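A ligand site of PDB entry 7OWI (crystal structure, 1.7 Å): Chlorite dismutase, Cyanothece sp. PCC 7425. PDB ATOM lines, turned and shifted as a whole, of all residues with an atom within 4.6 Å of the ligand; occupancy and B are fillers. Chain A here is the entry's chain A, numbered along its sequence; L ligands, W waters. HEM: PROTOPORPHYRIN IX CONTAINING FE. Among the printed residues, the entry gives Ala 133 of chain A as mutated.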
ATOM      1  N   ASN A  64       7.710  23.029  -0.074  1.00  0.00           N
ATOM      2  CA  ASN A  64       8.362  23.984  -0.942  1.00  0.00           C
ATOM      3  C   ASN A  64       9.434  24.764  -0.197  1.00  0.00           C
ATOM      4  O   ASN A  64       9.472  24.835   1.030  1.00  0.00           O
ATOM      5  CB  ASN A  64       7.351  24.948  -1.537  1.00  0.00           C
ATOM      6  CG  ASN A  64       6.584  25.717  -0.477  1.00  0.00           C
ATOM      7  OD1 ASN A  64       5.648  25.209   0.116  1.00  0.00           O
ATOM      8  ND2 ASN A  64       7.002  26.964  -0.228  1.00  0.00           N
ATOM      9  N   ILE A  65      10.323  25.382  -0.977  1.00  0.00           N
ATOM     10  CA  ILE A  65      11.384  26.217  -0.431  1.00  0.00           C
ATOM     11  C   ILE A  65      10.788  27.434   0.274  1.00  0.00           C
ATOM     12  O   ILE A  65       9.880  28.108  -0.225  1.00  0.00           O
ATOM     13  CB  ILE A  65      12.318  26.648  -1.576  1.00  0.00           C
ATOM     14  CG1 ILE A  65      13.095  25.431  -2.099  1.00  0.00           C
ATOM     15  CG2 ILE A  65      13.270  27.760  -1.145  1.00  0.00           C
ATOM     16  CD1 ILE A  65      14.031  24.792  -1.099  1.00  0.00           C
ATOM     17  N   ARG A  66      11.340  27.720   1.464  1.00  0.00           N
ATOM     18  CA  ARG A  66      10.910  28.833   2.301  1.00  0.00           C
ATOM     19  C   ARG A  66      11.892  29.989   2.368  1.00  0.00           C
ATOM     20  O   ARG A  66      11.472  31.104   2.677  1.00  0.00           O
ATOM     21  CB  ARG A  66      10.690  28.331   3.744  1.00  0.00           C
ATOM     22  CG  ARG A  66       9.845  27.080   3.840  1.00  0.00           C
ATOM     23  CD  ARG A  66       8.497  27.254   3.150  1.00  0.00           C
ATOM     24  NE  ARG A  66       7.667  26.052   3.239  1.00  0.00           N
ATOM     25  CZ  ARG A  66       6.947  25.724   4.309  1.00  0.00           C
ATOM     26  NH1 ARG A  66       6.890  26.513   5.359  1.00  0.00           N
ATOM     27  NH2 ARG A  66       6.257  24.579   4.290  1.00  0.00           N
ATOM     28  N   TYR A  67      13.183  29.764   2.105  1.00  0.00           N
ATOM     29  CA  TYR A  67      14.199  30.788   2.312  1.00  0.00           C
ATOM     30  C   TYR A  67      15.207  30.856   1.173  1.00  0.00           C
ATOM     31  O   TYR A  67      15.661  31.940   0.802  1.00  0.00           O
ATOM     32  CB  TYR A  67      14.958  30.525   3.629  1.00  0.00           C
ATOM     33  CG  TYR A  67      14.086  30.691   4.860  1.00  0.00           C
ATOM     34  CD1 TYR A  67      13.594  31.932   5.194  1.00  0.00           C
ATOM     35  CD2 TYR A  67      13.749  29.596   5.660  1.00  0.00           C
ATOM     36  CE1 TYR A  67      12.769  32.097   6.315  1.00  0.00           C
ATOM     37  CE2 TYR A  67      12.932  29.761   6.769  1.00  0.00           C
ATOM     38  CZ  TYR A  67      12.443  31.025   7.081  1.00  0.00           C
ATOM     39  OH  TYR A  67      11.632  31.196   8.193  1.00  0.00           O
ATOM     40  N   ALA A  68      15.608  29.683   0.644  1.00  0.00           N
ATOM     41  CA  ALA A  68      16.666  29.667  -0.363  1.00  0.00           C
ATOM     42  C   ALA A  68      16.287  30.484  -1.602  1.00  0.00           C
ATOM     43  O   ALA A  68      15.169  30.391  -2.102  1.00  0.00           O
ATOM     44  CB  ALA A  68      16.980  28.245  -0.789  1.00  0.00           C
ATOM     45  N   LEU A  76      23.061  24.155  -4.416  1.00  0.00           N
ATOM     46  CA  LEU A  76      22.694  22.947  -3.682  1.00  0.00           C
ATOM     47  C   LEU A  76      22.473  21.780  -4.629  1.00  0.00           C
ATOM     48  O   LEU A  76      23.054  20.704  -4.460  1.00  0.00           O
ATOM     49  CB  LEU A  76      21.427  23.182  -2.863  1.00  0.00           C
ATOM     50  CG  LEU A  76      21.498  24.063  -1.628  1.00  0.00           C
ATOM     51  CD1 LEU A  76      20.070  24.382  -1.165  1.00  0.00           C
ATOM     52  CD2 LEU A  76      22.264  23.368  -0.529  1.00  0.00           C
ATOM     53  N   ILE A  94      17.650  14.331  13.254  1.00  0.00           N
ATOM     54  CA  ILE A  94      17.712  15.411  14.234  1.00  0.00           C
ATOM     55  C   ILE A  94      16.406  16.205  14.211  1.00  0.00           C
ATOM     56  O   ILE A  94      16.248  17.154  13.419  1.00  0.00           O
ATOM     57  CB  ILE A  94      18.909  16.336  13.999  1.00  0.00           C
ATOM     58  CG1 ILE A  94      20.194  15.530  13.970  1.00  0.00           C
ATOM     59  CG2 ILE A  94      18.984  17.389  15.091  1.00  0.00           C
ATOM     60  CD1 ILE A  94      21.471  16.377  13.715  1.00  0.00           C
ATOM     61  N   ILE A  96      13.961  19.057  15.471  1.00  0.00           N
ATOM     62  CA  ILE A  96      14.273  20.394  15.961  1.00  0.00           C
ATOM     63  C   ILE A  96      12.994  21.182  16.154  1.00  0.00           C
ATOM     64  O   ILE A  96      12.079  21.117  15.323  1.00  0.00           O
ATOM     65  CB  ILE A  96      15.206  21.145  14.987  1.00  0.00           C
ATOM     66  CG1 ILE A  96      16.638  20.607  15.107  1.00  0.00           C
ATOM     67  CG2 ILE A  96      15.200  22.645  15.278  1.00  0.00           C
ATOM     68  CD1 ILE A  96      17.486  20.858  13.873  1.00  0.00           C
ATOM     69  N   LYS A  98      11.781  25.242  17.136  1.00  0.00           N
ATOM     70  CA  LYS A  98      12.178  26.632  17.285  1.00  0.00           C
ATOM     71  C   LYS A  98      11.157  27.356  18.155  1.00  0.00           C
ATOM     72  O   LYS A  98      10.019  26.906  18.321  1.00  0.00           O
ATOM     73  CB  LYS A  98      12.290  27.323  15.921  1.00  0.00           C
ATOM     74  CG  LYS A  98      13.502  26.796  15.093  1.00  0.00           C
ATOM     75  CD  LYS A  98      13.672  27.610  13.810  1.00  0.00           C
ATOM     76  CE  LYS A  98      14.958  27.245  13.098  1.00  0.00           C
ATOM     77  NZ  LYS A  98      15.211  28.147  11.919  1.00  0.00           N
ATOM     78  N   TRP A 102      10.676  32.993  17.346  1.00  0.00           N
ATOM     79  CA  TRP A 102      11.062  32.808  15.950  1.00  0.00           C
ATOM     80  C   TRP A 102       9.839  32.862  15.045  1.00  0.00           C
ATOM     81  O   TRP A 102       9.813  33.582  14.041  1.00  0.00           O
ATOM     82  CB  TRP A 102      11.790  31.479  15.786  1.00  0.00           C
ATOM     83  CG  TRP A 102      11.992  31.060  14.383  1.00  0.00           C
ATOM     84  CD1 TRP A 102      11.181  30.250  13.653  1.00  0.00           C
ATOM     85  CD2 TRP A 102      13.056  31.466  13.505  1.00  0.00           C
ATOM     86  NE1 TRP A 102      11.678  30.116  12.383  1.00  0.00           N
ATOM     87  CE2 TRP A 102      12.822  30.856  12.263  1.00  0.00           C
ATOM     88  CE3 TRP A 102      14.182  32.278  13.642  1.00  0.00           C
ATOM     89  CZ2 TRP A 102      13.684  31.019  11.173  1.00  0.00           C
ATOM     90  CZ3 TRP A 102      15.016  32.444  12.569  1.00  0.00           C
ATOM     91  CH2 TRP A 102      14.771  31.816  11.353  1.00  0.00           C
ATOM     92  N   PHE A 114      18.561  33.554   9.150  1.00  0.00           N
ATOM     93  CA  PHE A 114      18.892  32.254   8.572  1.00  0.00           C
ATOM     94  C   PHE A 114      20.148  32.325   7.717  1.00  0.00           C
ATOM     95  O   PHE A 114      21.041  31.491   7.850  1.00  0.00           O
ATOM     96  CB  PHE A 114      17.684  31.750   7.761  1.00  0.00           C
ATOM     97  CG  PHE A 114      17.940  30.503   6.988  1.00  0.00           C
ATOM     98  CD1 PHE A 114      17.846  29.265   7.607  1.00  0.00           C
ATOM     99  CD2 PHE A 114      18.261  30.557   5.639  1.00  0.00           C
ATOM    100  CE1 PHE A 114      18.077  28.106   6.902  1.00  0.00           C
ATOM    101  CE2 PHE A 114      18.494  29.386   4.927  1.00  0.00           C
ATOM    102  CZ  PHE A 114      18.404  28.179   5.563  1.00  0.00           C
ATOM    103  N   HIS A 120      23.511  29.797   6.977  1.00  0.00           N
ATOM    104  CA  HIS A 120      23.106  28.394   7.090  1.00  0.00           C
ATOM    105  C   HIS A 120      23.426  27.629   5.806  1.00  0.00           C
ATOM    106  O   HIS A 120      24.059  26.575   5.843  1.00  0.00           O
ATOM    107  CB  HIS A 120      21.641  28.300   7.376  1.00  0.00           C
ATOM    108  CG  HIS A 120      21.107  26.932   7.653  1.00  0.00           C
ATOM    109  ND1 HIS A 120      20.775  26.497   8.913  1.00  0.00           N
ATOM    110  CD2 HIS A 120      20.910  25.880   6.832  1.00  0.00           C
ATOM    111  CE1 HIS A 120      20.324  25.263   8.840  1.00  0.00           C
ATOM    112  NE2 HIS A 120      20.423  24.840   7.598  1.00  0.00           N
ATOM    113  N   THR A 121      22.993  28.155   4.664  1.00  0.00           N
ATOM    114  CA  THR A 121      23.220  27.450   3.402  1.00  0.00           C
ATOM    115  C   THR A 121      24.681  27.448   3.000  1.00  0.00           C
ATOM    116  O   THR A 121      25.217  26.411   2.586  1.00  0.00           O
ATOM    117  CB  THR A 121      22.370  28.069   2.288  1.00  0.00           C
ATOM    118  OG1 THR A 121      21.013  28.156   2.709  1.00  0.00           O
ATOM    119  CG2 THR A 121      22.458  27.218   1.021  1.00  0.00           C
ATOM    120  N   GLY A 124      26.489  24.954   5.182  1.00  0.00           N
ATOM    121  CA  GLY A 124      26.104  23.600   4.829  1.00  0.00           C
ATOM    122  C   GLY A 124      26.682  23.145   3.497  1.00  0.00           C
ATOM    123  O   GLY A 124      27.041  21.974   3.348  1.00  0.00           O
ATOM    124  N   LEU A 125      26.769  24.051   2.525  1.00  0.00           N
ATOM    125  CA  LEU A 125      27.269  23.658   1.214  1.00  0.00           C
ATOM    126  C   LEU A 125      28.693  23.121   1.289  1.00  0.00           C
ATOM    127  O   LEU A 125      29.109  22.332   0.414  1.00  0.00           O
ATOM    128  CB  LEU A 125      27.221  24.832   0.242  1.00  0.00           C
ATOM    129  CG  LEU A 125      25.928  25.000  -0.563  1.00  0.00           C
ATOM    130  CD1 LEU A 125      25.950  26.337  -1.326  1.00  0.00           C
ATOM    131  CD2 LEU A 125      25.746  23.853  -1.537  1.00  0.00           C
ATOM    132  N   LEU A 128      28.568  19.211   1.669  1.00  0.00           N
ATOM    133  CA  LEU A 128      28.222  18.376   0.525  1.00  0.00           C
ATOM    134  C   LEU A 128      29.416  18.305  -0.423  1.00  0.00           C
ATOM    135  O   LEU A 128      30.240  19.224  -0.460  1.00  0.00           O
ATOM    136  CB  LEU A 128      27.016  18.946  -0.197  1.00  0.00           C
ATOM    137  CG  LEU A 128      25.848  19.468   0.647  1.00  0.00           C
ATOM    138  CD1 LEU A 128      24.587  19.551  -0.190  1.00  0.00           C
ATOM    139  CD2 LEU A 128      25.624  18.626   1.883  1.00  0.00           C
ATOM    140  N   VAL A 131      27.738  14.708   2.591  1.00  0.00           N
ATOM    141  CA  VAL A 131      26.574  14.532   3.456  1.00  0.00           C
ATOM    142  C   VAL A 131      25.312  14.732   2.620  1.00  0.00           C
ATOM    143  O   VAL A 131      25.093  15.812   2.078  1.00  0.00           O
ATOM    144  CB  VAL A 131      26.595  15.514   4.640  1.00  0.00           C
ATOM    145  CG1 VAL A 131      25.318  15.382   5.483  1.00  0.00           C
ATOM    146  CG2 VAL A 131      27.845  15.303   5.493  1.00  0.00           C
ATOM    147  N   ALA A 133      21.552  15.518   2.821  1.00  0.00           N
ATOM    148  CA  ALA A 133      20.740  16.189   3.814  1.00  0.00           C
ATOM    149  C   ALA A 133      19.330  16.371   3.276  1.00  0.00           C
ATOM    150  O   ALA A 133      19.147  16.722   2.110  1.00  0.00           O
ATOM    151  CB  ALA A 133      21.346  17.544   4.193  1.00  0.00           C
ATOM    152  N   LEU A 135      15.110  17.697   4.543  1.00  0.00           N
ATOM    153  CA  LEU A 135      14.325  18.485   5.488  1.00  0.00           C
ATOM    154  C   LEU A 135      12.858  18.114   5.359  1.00  0.00           C
ATOM    155  O   LEU A 135      12.309  18.101   4.253  1.00  0.00           O
ATOM    156  CB  LEU A 135      14.492  19.987   5.211  1.00  0.00           C
ATOM    157  CG  LEU A 135      13.638  20.956   6.014  1.00  0.00           C
ATOM    158  CD1 LEU A 135      14.026  20.839   7.514  1.00  0.00           C
ATOM    159  CD2 LEU A 135      13.811  22.381   5.514  1.00  0.00           C
ATOM    160  N   PHE A 147      10.637  20.552  12.829  1.00  0.00           N
ATOM    161  CA  PHE A 147      11.327  20.036  11.672  1.00  0.00           C
ATOM    162  C   PHE A 147      11.901  18.661  12.012  1.00  0.00           C
ATOM    163  O   PHE A 147      12.258  18.389  13.163  1.00  0.00           O
ATOM    164  CB  PHE A 147      12.480  20.943  11.242  1.00  0.00           C
ATOM    165  CG  PHE A 147      12.095  22.373  11.022  1.00  0.00           C
ATOM    166  CD1 PHE A 147      11.445  22.751   9.848  1.00  0.00           C
ATOM    167  CD2 PHE A 147      12.358  23.318  11.960  1.00  0.00           C
ATOM    168  CE1 PHE A 147      11.104  24.061   9.668  1.00  0.00           C
ATOM    169  CE2 PHE A 147      12.016  24.638  11.763  1.00  0.00           C
ATOM    170  CZ  PHE A 147      11.391  24.992  10.618  1.00  0.00           C
ATOM    171  N   THR A 149      15.089  16.694  10.444  1.00  0.00           N
ATOM    172  CA  THR A 149      16.221  16.780   9.528  1.00  0.00           C
ATOM    173  C   THR A 149      16.918  15.437   9.476  1.00  0.00           C
ATOM    174  O   THR A 149      17.027  14.740  10.486  1.00  0.00           O
ATOM    175  CB  THR A 149      17.193  17.904   9.929  1.00  0.00           C
ATOM    176  OG1 THR A 149      17.788  17.635  11.187  1.00  0.00           O
ATOM    177  CG2 THR A 149      16.449  19.230   9.987  1.00  0.00           C
ATOM    178  N   PHE A 151      20.192  13.101   7.709  1.00  0.00           N
ATOM    179  CA  PHE A 151      21.546  13.128   7.159  1.00  0.00           C
ATOM    180  C   PHE A 151      22.051  11.709   7.032  1.00  0.00           C
ATOM    181  O   PHE A 151      21.805  10.871   7.909  1.00  0.00           O
ATOM    182  CB  PHE A 151      22.477  13.924   8.069  1.00  0.00           C
ATOM    183  CG  PHE A 151      21.929  15.264   8.422  1.00  0.00           C
ATOM    184  CD1 PHE A 151      22.119  16.332   7.597  1.00  0.00           C
ATOM    185  CD2 PHE A 151      21.171  15.422   9.579  1.00  0.00           C
ATOM    186  CE1 PHE A 151      21.582  17.584   7.906  1.00  0.00           C
ATOM    187  CE2 PHE A 151      20.650  16.660   9.914  1.00  0.00           C
ATOM    188  CZ  PHE A 151      20.846  17.733   9.068  1.00  0.00           C
ATOM    189  N   PHE A 161      31.031  15.846   9.812  1.00  0.00           N
ATOM    190  CA  PHE A 161      29.652  16.108  10.188  1.00  0.00           C
ATOM    191  C   PHE A 161      29.579  16.684  11.592  1.00  0.00           C
ATOM    192  O   PHE A 161      28.781  17.572  11.859  1.00  0.00           O
ATOM    193  CB  PHE A 161      28.812  14.839  10.086  1.00  0.00           C
ATOM    194  CG  PHE A 161      27.355  15.072  10.346  1.00  0.00           C
ATOM    195  CD1 PHE A 161      26.585  15.767   9.447  1.00  0.00           C
ATOM    196  CD2 PHE A 161      26.774  14.618  11.525  1.00  0.00           C
ATOM    197  CE1 PHE A 161      25.242  15.996   9.682  1.00  0.00           C
ATOM    198  CE2 PHE A 161      25.432  14.841  11.769  1.00  0.00           C
ATOM    199  CZ  PHE A 161      24.668  15.542  10.849  1.00  0.00           C
ATOM    200  N   LEU A 164      30.347  20.262  11.299  1.00  0.00           N
ATOM    201  CA  LEU A 164      29.182  20.992  10.812  1.00  0.00           C
ATOM    202  C   LEU A 164      28.228  21.281  11.951  1.00  0.00           C
ATOM    203  O   LEU A 164      27.775  22.414  12.144  1.00  0.00           O
ATOM    204  CB  LEU A 164      28.486  20.169   9.733  1.00  0.00           C
ATOM    205  CG  LEU A 164      27.104  20.650   9.244  1.00  0.00           C
ATOM    206  CD1 LEU A 164      27.181  22.028   8.666  1.00  0.00           C
ATOM    207  CD2 LEU A 164      26.563  19.630   8.242  1.00  0.00           C
ATOM    208  N   LEU A 165      27.924  20.267  12.761  1.00  0.00           N
ATOM    209  CA  LEU A 165      27.037  20.478  13.904  1.00  0.00           C
ATOM    210  C   LEU A 165      27.592  21.547  14.842  1.00  0.00           C
ATOM    211  O   LEU A 165      26.851  22.410  15.310  1.00  0.00           O
ATOM    212  CB  LEU A 165      26.855  19.173  14.667  1.00  0.00           C
ATOM    213  CG  LEU A 165      26.037  18.084  13.955  1.00  0.00           C
ATOM    214  CD1 LEU A 165      26.014  16.823  14.798  1.00  0.00           C
ATOM    215  CD2 LEU A 165      24.617  18.555  13.664  1.00  0.00           C
ATOM    216  N   MET A 168      26.843  24.951  13.287  1.00  0.00           N
ATOM    217  CA  MET A 168      25.445  25.355  13.282  1.00  0.00           C
ATOM    218  C   MET A 168      24.934  25.682  14.683  1.00  0.00           C
ATOM    219  O   MET A 168      24.160  26.639  14.859  1.00  0.00           O
ATOM    220  CB  MET A 168      24.585  24.271  12.636  1.00  0.00           C
ATOM    221  CG  MET A 168      25.194  23.805  11.329  1.00  0.00           C
ATOM    222  SD  MET A 168      23.986  23.294  10.137  1.00  0.00           S
ATOM    223  CE  MET A 168      23.543  24.889   9.507  1.00  0.00           C
ATOM    224  N   ARG A 169      25.366  24.909  15.685  1.00  0.00           N
ATOM    225  CA  ARG A 169      24.859  25.141  17.039  1.00  0.00           C
ATOM    226  C   ARG A 169      25.369  26.445  17.631  1.00  0.00           C
ATOM    227  O   ARG A 169      24.823  26.923  18.633  1.00  0.00           O
ATOM    228  CB  ARG A 169      25.242  23.953  17.947  1.00  0.00           C
ATOM    229  CG  ARG A 169      24.195  22.833  18.037  1.00  0.00           C
ATOM    230  CD  ARG A 169      23.947  22.159  16.746  1.00  0.00           C
ATOM    231  NE  ARG A 169      23.041  21.001  16.858  1.00  0.00           N
ATOM    232  CZ  ARG A 169      23.403  19.784  17.269  1.00  0.00           C
ATOM    233  NH1 ARG A 169      24.643  19.506  17.648  1.00  0.00           N
ATOM    234  NH2 ARG A 169      22.499  18.812  17.270  1.00  0.00           N
ATOM    235  N   GLU A 173      21.011  31.668  14.353  1.00  0.00           N
ATOM    236  CA  GLU A 173      19.784  30.910  14.152  1.00  0.00           C
ATOM    237  C   GLU A 173      19.514  29.970  15.322  1.00  0.00           C
ATOM    238  O   GLU A 173      18.364  29.773  15.725  1.00  0.00           O
ATOM    239  CB  GLU A 173      19.873  30.109  12.845  1.00  0.00           C
ATOM    240  CG  GLU A 173      18.574  29.426  12.427  1.00  0.00           C
ATOM    241  CD  GLU A 173      18.752  28.448  11.274  1.00  0.00           C
ATOM    242  OE1 GLU A 173      17.777  27.765  10.930  1.00  0.00           O
ATOM    243  OE2 GLU A 173      19.880  28.354  10.742  1.00  0.00           O
ATOM    244  N   TRP A 174      20.553  29.337  15.845  1.00  0.00           N
ATOM    245  CA  TRP A 174      20.336  28.350  16.898  1.00  0.00           C
ATOM    246  C   TRP A 174      19.966  28.960  18.234  1.00  0.00           C
ATOM    247  O   TRP A 174      19.520  28.237  19.129  1.00  0.00           O
ATOM    248  CB  TRP A 174      21.567  27.446  17.073  1.00  0.00           C
ATOM    249  CG  TRP A 174      21.264  26.049  16.628  1.00  0.00           C
ATOM    250  CD1 TRP A 174      21.122  24.933  17.431  1.00  0.00           C
ATOM    251  CD2 TRP A 174      20.992  25.608  15.294  1.00  0.00           C
ATOM    252  NE1 TRP A 174      20.793  23.856  16.667  1.00  0.00           N
ATOM    253  CE2 TRP A 174      20.719  24.230  15.350  1.00  0.00           C
ATOM    254  CE3 TRP A 174      20.942  26.252  14.057  1.00  0.00           C
ATOM    255  CZ2 TRP A 174      20.403  23.493  14.216  1.00  0.00           C
ATOM    256  CZ3 TRP A 174      20.648  25.519  12.935  1.00  0.00           C
ATOM    257  CH2 TRP A 174      20.386  24.161  13.015  1.00  0.00           C
ATOM    258  N   GLU A 180      15.910  19.906  20.755  1.00  0.00           N
ATOM    259  CA  GLU A 180      16.742  19.254  19.748  1.00  0.00           C
ATOM    260  C   GLU A 180      17.188  17.905  20.293  1.00  0.00           C
ATOM    261  O   GLU A 180      17.574  17.802  21.461  1.00  0.00           O
ATOM    262  CB  GLU A 180      17.945  20.115  19.402  1.00  0.00           C
ATOM    263  CG  GLU A 180      18.800  19.592  18.272  1.00  0.00           C
ATOM    264  CD  GLU A 180      19.777  20.621  17.722  1.00  0.00           C
ATOM    265  OE1 GLU A 180      19.965  21.667  18.375  1.00  0.00           O
ATOM    266  OE2 GLU A 180      20.356  20.375  16.634  1.00  0.00           O
HETATM  267  CHA HEM L   1      16.747  24.440   6.316  1.00  0.00           C
HETATM  268  CHB HEM L   1      20.770  23.703   3.699  1.00  0.00           C
HETATM  269  CHC HEM L   1      22.634  21.066   7.350  1.00  0.00           C
HETATM  270  CHD HEM L   1      18.717  22.050  10.060  1.00  0.00           C
HETATM  271  C1A HEM L   1      17.680  24.507   5.314  1.00  0.00           C
HETATM  272  C2A HEM L   1      17.563  25.223   4.057  1.00  0.00           C
HETATM  273  C3A HEM L   1      18.664  25.027   3.348  1.00  0.00           C
HETATM  274  C4A HEM L   1      19.539  24.149   4.102  1.00  0.00           C
HETATM  275  CMA HEM L   1      18.992  25.580   1.950  1.00  0.00           C
HETATM  276  CAA HEM L   1      16.338  26.108   3.659  1.00  0.00           C
HETATM  277  CBA HEM L   1      15.298  25.305   2.931  1.00  0.00           C
HETATM  278  CGA HEM L   1      14.177  26.262   2.542  1.00  0.00           C
HETATM  279  O1A HEM L   1      14.507  27.343   2.005  1.00  0.00           O
HETATM  280  O2A HEM L   1      12.998  25.927   2.759  1.00  0.00           O
HETATM  281  C1B HEM L   1      21.571  22.842   4.412  1.00  0.00           C
HETATM  282  C2B HEM L   1      22.751  22.168   3.922  1.00  0.00           C
HETATM  283  C3B HEM L   1      23.251  21.426   4.913  1.00  0.00           C
HETATM  284  C4B HEM L   1      22.444  21.632   6.092  1.00  0.00           C
HETATM  285  CMB HEM L   1      23.266  22.258   2.469  1.00  0.00           C
HETATM  286  CAB HEM L   1      24.489  20.520   4.769  1.00  0.00           C
HETATM  287  CBB HEM L   1      24.582  19.392   5.459  1.00  0.00           C
HETATM  288  C1C HEM L   1      21.769  21.151   8.415  1.00  0.00           C
HETATM  289  C2C HEM L   1      22.009  20.655   9.758  1.00  0.00           C
HETATM  290  C3C HEM L   1      20.923  20.915  10.516  1.00  0.00           C
HETATM  291  C4C HEM L   1      19.962  21.613   9.672  1.00  0.00           C
HETATM  292  CMC HEM L   1      23.307  19.931  10.165  1.00  0.00           C
HETATM  293  CAC HEM L   1      20.654  20.579  12.006  1.00  0.00           C
HETATM  294  CBC HEM L   1      21.624  20.267  12.849  1.00  0.00           C
HETATM  295  C1D HEM L   1      17.845  22.787   9.290  1.00  0.00           C
HETATM  296  C2D HEM L   1      16.548  23.301   9.707  1.00  0.00           C
HETATM  297  C3D HEM L   1      16.014  23.971   8.663  1.00  0.00           C
HETATM  298  C4D HEM L   1      16.943  23.886   7.569  1.00  0.00           C
HETATM  299  CMD HEM L   1      15.966  23.117  11.097  1.00  0.00           C
HETATM  300  CAD HEM L   1      14.659  24.700   8.628  1.00  0.00           C
HETATM  301  CBD HEM L   1      14.897  26.188   8.900  1.00  0.00           C
HETATM  302  CGD HEM L   1      13.581  26.904   8.960  1.00  0.00           C
HETATM  303  O1D HEM L   1      13.407  27.707   9.912  1.00  0.00           O
HETATM  304  O2D HEM L   1      12.701  26.672   8.082  1.00  0.00           O
HETATM  305  NA  HEM L   1      18.897  23.845   5.296  1.00  0.00           N
HETATM  306  NB  HEM L   1      21.430  22.490   5.762  1.00  0.00           N
HETATM  307  NC  HEM L   1      20.518  21.743   8.404  1.00  0.00           N
HETATM  308  ND  HEM L   1      18.043  23.143   7.972  1.00  0.00           N
HETATM  309 FE   HEM L   1      19.786  22.942   6.915  1.00  0.00          FE
HETATM  310  O   HOH W   1      12.769  25.729   5.598  1.00  0.00           O
HETATM  311  O   HOH W   2       9.889  27.327   7.805  1.00  0.00           O
HETATM  312  O   HOH W   3      11.228  29.057   9.667  1.00  0.00           O
HETATM  313  O   HOH W   4      18.641  20.862   6.031  1.00  0.00           O
HETATM  314  O   HOH W   5      11.621  23.667   2.634  1.00  0.00           O
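FE of the ligand is bound by NE2 of His 120 (2.1 Å). The side-chain amino group of Lys 98 lies within salt-bridge range of an oxygen (O1D) of the ligand (2.7 Å). An oxygen (O2A) of the ligand sits at hydrogen-bond distance from the backbone NH (N) of Arg 66 (2.8 Å). An oxygen (O1A) of the ligand sits at hydrogen-bond distance from the backbone NH (N) of Tyr 67 (2.8 Å). The backbone NH of Ala 68 sits at hydrogen-bond distance from an oxygen (O1A) of the ligand, at 2.9 Å.
NZ of Lys 98 is in salt-bridge range of OE1 of Glu 173. The guanidinium group (NE) of Arg 66 lies within hydrogen-bond range of the backbone carbonyl oxygen (O) of Asn 64. OE2 of Glu 180 is in salt-bridge range of NH2 of Arg 169. A ring nitrogen (ND1) of His 120 sits at hydrogen-bond distance from the side-chain carboxylate (OE2) of Glu 173, at 2.8 Å. The backbone carbonyl oxygen (O) of Ile 96 sits at hydrogen-bond distance from the backbone NH (N) of Phe 147 (2.9 Å). The side-chain hydroxyl of Thr 149 is in hydrogen-bond range of the backbone carbonyl oxygen of Ile 94 (2.8 Å). NE1 of Trp 174 sits at hydrogen-bond distance from OE1 of Glu 180, at 2.9 Å. The backbone NH of His 120 is in hydrogen-bond range of the backbone carbonyl oxygen of Phe 114, 3.1 Å away.
Residues that only touch the ligand: Ile 65 (3.4 Å), Leu 76 (3.4 Å), Ile 94 (3.99 Å), Ile 96 (3.7 Å), Trp 102 (3.6 Å), Phe 114 (3.4 Å), Thr 121 (3.4 Å), Gly 124 (3.3 Å), Leu 125 (3.9 Å), Leu 128 (3.6 Å), Ala 133 (3.9 Å), Leu 135 (3.7 Å), Phe 147 (3.3 Å), Thr 149 (3.6 Å), Phe 151 (3.2 Å), Leu 164 (3.4 Å), Leu 165 (3.5 Å), Met 168 (3.3 Å), Glu 173 (3.9 Å), Trp 174 (3.7 Å) and Glu 180 (3.99 Å). Hydrophobic or aromatic side chains within 4 Å of the ligand: Ile 65, Tyr 67, Ala 68, Leu 76, Ile 94, Ile 96, Trp 102, Phe 114, His 120, Leu 128, Ala 133, Leu 135, Phe 147, Phe 151, Leu 164, Leu 165, Met 168 and Trp 174. 26 residues have an atom within 4 Å of the ligand: Ile 65, Arg 66, Tyr 67, Ala 68, Leu 76, Ile 94, Ile 96, Lys 98, Trp 102, Phe 114, His 120, Thr 121, Gly 124, Leu 125, Leu 128, Ala 133, Leu 135, Phe 147, Thr 149, Phe 151, Leu 164, Leu 165, Met 168, Glu 173, Trp 174 and Glu 180.
Water W3 lies within hydrogen-bond range of an oxygen (O1D) of the ligand, the side-chain hydroxyl of Tyr 67 and the indole nitrogen of Trp 102. Water W5 lies within hydrogen-bond range of an oxygen (O2A) of the ligand (2.6 Å) and the backbone carbonyl oxygen (O) of Asn 64 (2.9 Å).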
